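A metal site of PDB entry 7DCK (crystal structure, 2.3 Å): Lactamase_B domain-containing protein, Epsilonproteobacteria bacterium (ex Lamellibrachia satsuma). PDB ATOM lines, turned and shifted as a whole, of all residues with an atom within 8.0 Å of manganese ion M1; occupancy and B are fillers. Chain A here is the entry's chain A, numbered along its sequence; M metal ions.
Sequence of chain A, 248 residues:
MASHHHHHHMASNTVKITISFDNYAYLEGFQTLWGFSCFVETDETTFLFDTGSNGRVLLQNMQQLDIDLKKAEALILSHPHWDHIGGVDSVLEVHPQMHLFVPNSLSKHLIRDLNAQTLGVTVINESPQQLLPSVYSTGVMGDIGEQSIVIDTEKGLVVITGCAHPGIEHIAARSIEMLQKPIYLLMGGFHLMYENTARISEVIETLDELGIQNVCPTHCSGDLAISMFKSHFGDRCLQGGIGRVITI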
ATOM      1  N   TRP A  34      30.860  -1.504  28.181  1.00  0.00           N
ATOM      2  CA  TRP A  34      29.415  -1.621  28.066  1.00  0.00           C
ATOM      3  C   TRP A  34      28.723  -0.421  28.712  1.00  0.00           C
ATOM      4  O   TRP A  34      28.831  -0.214  29.927  1.00  0.00           O
ATOM      5  CB  TRP A  34      28.912  -2.910  28.709  1.00  0.00           C
ATOM      6  CG  TRP A  34      27.498  -3.203  28.337  1.00  0.00           C
ATOM      7  CD1 TRP A  34      26.390  -2.988  29.101  1.00  0.00           C
ATOM      8  CD2 TRP A  34      27.035  -3.733  27.093  1.00  0.00           C
ATOM      9  NE1 TRP A  34      25.261  -3.370  28.415  1.00  0.00           N
ATOM     10  CE2 TRP A  34      25.633  -3.834  27.175  1.00  0.00           C
ATOM     11  CE3 TRP A  34      27.664  -4.150  25.919  1.00  0.00           C
ATOM     12  CZ2 TRP A  34      24.852  -4.328  26.138  1.00  0.00           C
ATOM     13  CZ3 TRP A  34      26.889  -4.632  24.885  1.00  0.00           C
ATOM     14  CH2 TRP A  34      25.498  -4.722  25.000  1.00  0.00           C
ATOM     15  N   ASP A  50      23.077  10.543  29.871  1.00  0.00           N
ATOM     16  CA  ASP A  50      23.634   9.350  30.497  1.00  0.00           C
ATOM     17  C   ASP A  50      25.141   9.477  30.698  1.00  0.00           C
ATOM     18  O   ASP A  50      25.777  10.403  30.184  1.00  0.00           O
ATOM     19  CB  ASP A  50      23.293   8.086  29.694  1.00  0.00           C
ATOM     20  CG  ASP A  50      21.862   7.635  29.930  1.00  0.00           C
ATOM     21  OD1 ASP A  50      21.220   8.154  30.862  1.00  0.00           O
ATOM     22  OD2 ASP A  50      21.371   6.760  29.184  1.00  0.00           O
ATOM     23  N   SER A  78      18.645   8.358  31.403  1.00  0.00           N
ATOM     24  CA  SER A  78      17.554   7.659  30.727  1.00  0.00           C
ATOM     25  C   SER A  78      16.851   6.685  31.655  1.00  0.00           C
ATOM     26  O   SER A  78      15.610   6.641  31.701  1.00  0.00           O
ATOM     27  CB  SER A  78      18.093   6.930  29.489  1.00  0.00           C
ATOM     28  OG  SER A  78      18.961   5.873  29.854  1.00  0.00           O
ATOM     29  N   HIS A  79      17.606   5.878  32.407  1.00  0.00           N
ATOM     30  CA  HIS A  79      17.037   4.871  33.290  1.00  0.00           C
ATOM     31  C   HIS A  79      18.076   4.383  34.296  1.00  0.00           C
ATOM     32  O   HIS A  79      19.260   4.726  34.150  1.00  0.00           O
ATOM     33  CB  HIS A  79      16.434   3.716  32.459  1.00  0.00           C
ATOM     34  CG  HIS A  79      17.442   2.871  31.742  1.00  0.00           C
ATOM     35  ND1 HIS A  79      18.230   3.353  30.720  1.00  0.00           N
ATOM     36  CD2 HIS A  79      17.747   1.562  31.870  1.00  0.00           C
ATOM     37  CE1 HIS A  79      18.997   2.382  30.268  1.00  0.00           C
ATOM     38  NE2 HIS A  79      18.723   1.284  30.947  1.00  0.00           N
ATOM     39  N   PRO A  80      17.701   3.607  35.349  1.00  0.00           N
ATOM     40  CA  PRO A  80      18.640   3.394  36.468  1.00  0.00           C
ATOM     41  C   PRO A  80      19.667   2.284  36.289  1.00  0.00           C
ATOM     42  O   PRO A  80      20.271   1.870  37.276  1.00  0.00           O
ATOM     43  CB  PRO A  80      17.708   3.053  37.639  1.00  0.00           C
ATOM     44  CG  PRO A  80      16.310   3.197  37.128  1.00  0.00           C
ATOM     45  CD  PRO A  80      16.388   3.035  35.655  1.00  0.00           C
ATOM     46  N   HIS A  81      19.900   1.805  35.070  1.00  0.00           N
ATOM     47  CA  HIS A  81      20.809   0.679  34.902  1.00  0.00           C
ATOM     48  C   HIS A  81      22.266   1.097  35.087  1.00  0.00           C
ATOM     49  O   HIS A  81      22.664   2.208  34.706  1.00  0.00           O
ATOM     50  CB  HIS A  81      20.607   0.021  33.536  1.00  0.00           C
ATOM     51  CG  HIS A  81      19.411  -0.867  33.480  1.00  0.00           C
ATOM     52  ND1 HIS A  81      18.912  -1.387  32.296  1.00  0.00           N
ATOM     53  CD2 HIS A  81      18.593  -1.332  34.464  1.00  0.00           C
ATOM     54  CE1 HIS A  81      17.856  -2.128  32.559  1.00  0.00           C
ATOM     55  NE2 HIS A  81      17.632  -2.117  33.863  1.00  0.00           N
ATOM     56  N   TRP A  82      23.046   0.208  35.704  1.00  0.00           N
ATOM     57  CA  TRP A  82      24.426   0.485  36.078  1.00  0.00           C
ATOM     58  C   TRP A  82      25.246   1.088  34.936  1.00  0.00           C
ATOM     59  O   TRP A  82      26.123   1.932  35.170  1.00  0.00           O
ATOM     60  CB  TRP A  82      25.099  -0.802  36.553  1.00  0.00           C
ATOM     61  CG  TRP A  82      25.070  -1.865  35.493  1.00  0.00           C
ATOM     62  CD1 TRP A  82      24.038  -2.699  35.187  1.00  0.00           C
ATOM     63  CD2 TRP A  82      26.119  -2.167  34.553  1.00  0.00           C
ATOM     64  NE1 TRP A  82      24.384  -3.515  34.130  1.00  0.00           N
ATOM     65  CE2 TRP A  82      25.655  -3.206  33.724  1.00  0.00           C
ATOM     66  CE3 TRP A  82      27.410  -1.658  34.341  1.00  0.00           C
ATOM     67  CZ2 TRP A  82      26.428  -3.751  32.694  1.00  0.00           C
ATOM     68  CZ3 TRP A  82      28.178  -2.202  33.319  1.00  0.00           C
ATOM     69  CH2 TRP A  82      27.688  -3.240  32.508  1.00  0.00           C
ATOM     70  N   ASP A  83      24.981   0.665  33.705  1.00  0.00           N
ATOM     71  CA  ASP A  83      25.786   1.101  32.575  1.00  0.00           C
ATOM     72  C   ASP A  83      25.322   2.424  31.990  1.00  0.00           C
ATOM     73  O   ASP A  83      25.758   2.803  30.899  1.00  0.00           O
ATOM     74  CB  ASP A  83      25.792   0.017  31.494  1.00  0.00           C
ATOM     75  CG  ASP A  83      24.402  -0.323  31.006  1.00  0.00           C
ATOM     76  OD1 ASP A  83      23.495  -0.503  31.855  1.00  0.00           O
ATOM     77  OD2 ASP A  83      24.214  -0.397  29.786  1.00  0.00           O
ATOM     78  N   HIS A  84      24.434   3.148  32.689  1.00  0.00           N
ATOM     79  CA  HIS A  84      24.062   4.494  32.300  1.00  0.00           C
ATOM     80  C   HIS A  84      24.228   5.511  33.423  1.00  0.00           C
ATOM     81  O   HIS A  84      24.379   6.702  33.132  1.00  0.00           O
ATOM     82  CB  HIS A  84      22.604   4.535  31.796  1.00  0.00           C
ATOM     83  CG  HIS A  84      22.367   3.669  30.610  1.00  0.00           C
ATOM     84  ND1 HIS A  84      22.249   4.164  29.326  1.00  0.00           N
ATOM     85  CD2 HIS A  84      22.236   2.323  30.491  1.00  0.00           C
ATOM     86  CE1 HIS A  84      22.051   3.172  28.481  1.00  0.00           C
ATOM     87  NE2 HIS A  84      22.041   2.043  29.167  1.00  0.00           N
ATOM     88  N   ILE A 144      10.580  -0.971  33.244  1.00  0.00           N
ATOM     89  CA  ILE A 144      11.774  -0.511  33.945  1.00  0.00           C
ATOM     90  C   ILE A 144      11.686   0.983  34.241  1.00  0.00           C
ATOM     91  O   ILE A 144      12.297   1.472  35.198  1.00  0.00           O
ATOM     92  CB  ILE A 144      13.044  -0.867  33.148  1.00  0.00           C
ATOM     93  CG1 ILE A 144      13.112  -2.365  32.811  1.00  0.00           C
ATOM     94  CG2 ILE A 144      14.300  -0.474  33.919  1.00  0.00           C
ATOM     95  CD1 ILE A 144      12.543  -2.740  31.462  1.00  0.00           C
ATOM     96  N   GLU A 146      11.870   4.020  31.665  1.00  0.00           N
ATOM     97  CA  GLU A 146      12.924   4.660  30.891  1.00  0.00           C
ATOM     98  C   GLU A 146      12.354   5.847  30.128  1.00  0.00           C
ATOM     99  O   GLU A 146      11.288   5.750  29.503  1.00  0.00           O
ATOM    100  CB  GLU A 146      13.569   3.669  29.913  1.00  0.00           C
ATOM    101  CG  GLU A 146      14.582   4.314  28.980  1.00  0.00           C
ATOM    102  CD  GLU A 146      15.238   3.334  28.034  1.00  0.00           C
ATOM    103  OE1 GLU A 146      14.970   2.111  28.149  1.00  0.00           O
ATOM    104  OE2 GLU A 146      16.028   3.765  27.173  1.00  0.00           O
ATOM    105  N   GLY A 162      18.592   5.607  25.509  1.00  0.00           N
ATOM    106  CA  GLY A 162      19.610   4.854  26.229  1.00  0.00           C
ATOM    107  C   GLY A 162      19.688   3.398  25.804  1.00  0.00           C
ATOM    108  O   GLY A 162      20.587   3.018  25.053  1.00  0.00           O
ATOM    109  N   CYS A 163      18.781   2.552  26.300  1.00  0.00           N
ATOM    110  CA  CYS A 163      18.682   1.167  25.855  1.00  0.00           C
ATOM    111  C   CYS A 163      17.334   0.840  25.233  1.00  0.00           C
ATOM    112  O   CYS A 163      17.229  -0.201  24.582  1.00  0.00           O
ATOM    113  CB  CYS A 163      18.997   0.170  27.018  1.00  0.00           C
ATOM    114  SG  CYS A 163      19.909  -1.448  26.602  1.00  0.00           S
ATOM    115  N   ALA A 164      16.332   1.733  25.322  1.00  0.00           N
ATOM    116  CA  ALA A 164      15.058   1.580  24.605  1.00  0.00           C
ATOM    117  C   ALA A 164      14.310   0.325  25.039  1.00  0.00           C
ATOM    118  O   ALA A 164      13.701  -0.366  24.228  1.00  0.00           O
ATOM    119  CB  ALA A 164      15.247   1.579  23.081  1.00  0.00           C
ATOM    120  N   HIS A 165      14.342   0.041  26.341  1.00  0.00           N
ATOM    121  CA  HIS A 165      13.568  -1.062  26.899  1.00  0.00           C
ATOM    122  C   HIS A 165      12.087  -1.033  26.519  1.00  0.00           C
ATOM    123  O   HIS A 165      11.541  -2.107  26.206  1.00  0.00           O
ATOM    124  CB  HIS A 165      13.735  -1.089  28.424  1.00  0.00           C
ATOM    125  CG  HIS A 165      15.119  -1.438  28.875  1.00  0.00           C
ATOM    126  ND1 HIS A 165      15.619  -2.730  28.833  1.00  0.00           N
ATOM    127  CD2 HIS A 165      16.118  -0.672  29.381  1.00  0.00           C
ATOM    128  CE1 HIS A 165      16.857  -2.734  29.288  1.00  0.00           C
ATOM    129  NE2 HIS A 165      17.182  -1.507  29.638  1.00  0.00           N
ATOM    130  N   HIS A 191      18.066  -1.992  21.977  1.00  0.00           N
ATOM    131  CA  HIS A 191      17.751  -3.230  22.708  1.00  0.00           C
ATOM    132  C   HIS A 191      17.143  -4.298  21.809  1.00  0.00           C
ATOM    133  O   HIS A 191      16.115  -4.910  22.114  1.00  0.00           O
ATOM    134  CB  HIS A 191      16.807  -2.944  23.883  1.00  0.00           C
ATOM    135  CG  HIS A 191      17.144  -3.720  25.122  1.00  0.00           C
ATOM    136  ND1 HIS A 191      18.320  -3.558  25.812  1.00  0.00           N
ATOM    137  CD2 HIS A 191      16.441  -4.668  25.790  1.00  0.00           C
ATOM    138  CE1 HIS A 191      18.337  -4.371  26.856  1.00  0.00           C
ATOM    139  NE2 HIS A 191      17.205  -5.055  26.861  1.00  0.00           N
ATOM    140  N   HIS A 219      25.310   0.880  21.060  1.00  0.00           N
ATOM    141  CA  HIS A 219      25.179   0.323  22.414  1.00  0.00           C
ATOM    142  C   HIS A 219      24.519  -1.047  22.397  1.00  0.00           C
ATOM    143  O   HIS A 219      25.082  -2.001  21.847  1.00  0.00           O
ATOM    144  CB  HIS A 219      24.438   1.314  23.331  1.00  0.00           C
ATOM    145  CG  HIS A 219      24.259   0.817  24.740  1.00  0.00           C
ATOM    146  ND1 HIS A 219      25.248   0.118  25.405  1.00  0.00           N
ATOM    147  CD2 HIS A 219      23.202   0.872  25.580  1.00  0.00           C
ATOM    148  CE1 HIS A 219      24.809  -0.213  26.601  1.00  0.00           C
ATOM    149  NE2 HIS A 219      23.578   0.229  26.740  1.00  0.00           N
ATOM    150  N   CYS A 220      23.315  -1.184  22.983  1.00  0.00           N
ATOM    151  CA  CYS A 220      22.734  -2.518  23.137  1.00  0.00           C
ATOM    152  C   CYS A 220      21.895  -2.967  21.947  1.00  0.00           C
ATOM    153  O   CYS A 220      21.035  -3.826  22.085  1.00  0.00           O
ATOM    154  CB  CYS A 220      21.929  -2.585  24.445  1.00  0.00           C
ATOM    155  SG  CYS A 220      20.492  -1.411  24.628  1.00  0.00           S
HETATM  156 MN    MN M   1      19.225  -0.770  30.260  1.00  0.00          MN
HETATM  157 MN    MN M   2      22.399  -0.105  28.649  1.00  0.00          MN
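Merely in contact with manganese ion M1: Cys 163 (3.4 Å). The nearest printed residue that does not touch manganese ion M1 is His 84 (4.1 Å).
Manganese ion M1 is bound by ND1 of His 81, at 2.2 Å. NE2 of His 79 is bound to manganese ion M1 (2.2 Å). NE2 of His 165 is bound to manganese ion M1 (2.3 Å).
The side-chain hydroxyl of Ser 78 sits at hydrogen-bond distance from a ring nitrogen (ND1) of His 79, 2.8 Å away. A ring nitrogen (NE2) of His 191 lies close to a ring nitrogen (ND1) of His 165. The backbone NH (N) of His 165 sits at hydrogen-bond distance from the side-chain carboxylate (OE1) of Glu 146 (2.8 Å). ND1 of His 191 is in hydrogen-bond range of SG of Cys 163 (2.8 Å). The backbone NH (N) of Cys 163 is in hydrogen-bond range of the side-chain carboxylate (OE2) of Glu 146 (3.1 Å). SG of Cys 163 forms a disulfide with SG of Cys 220, 2.1 Å away.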
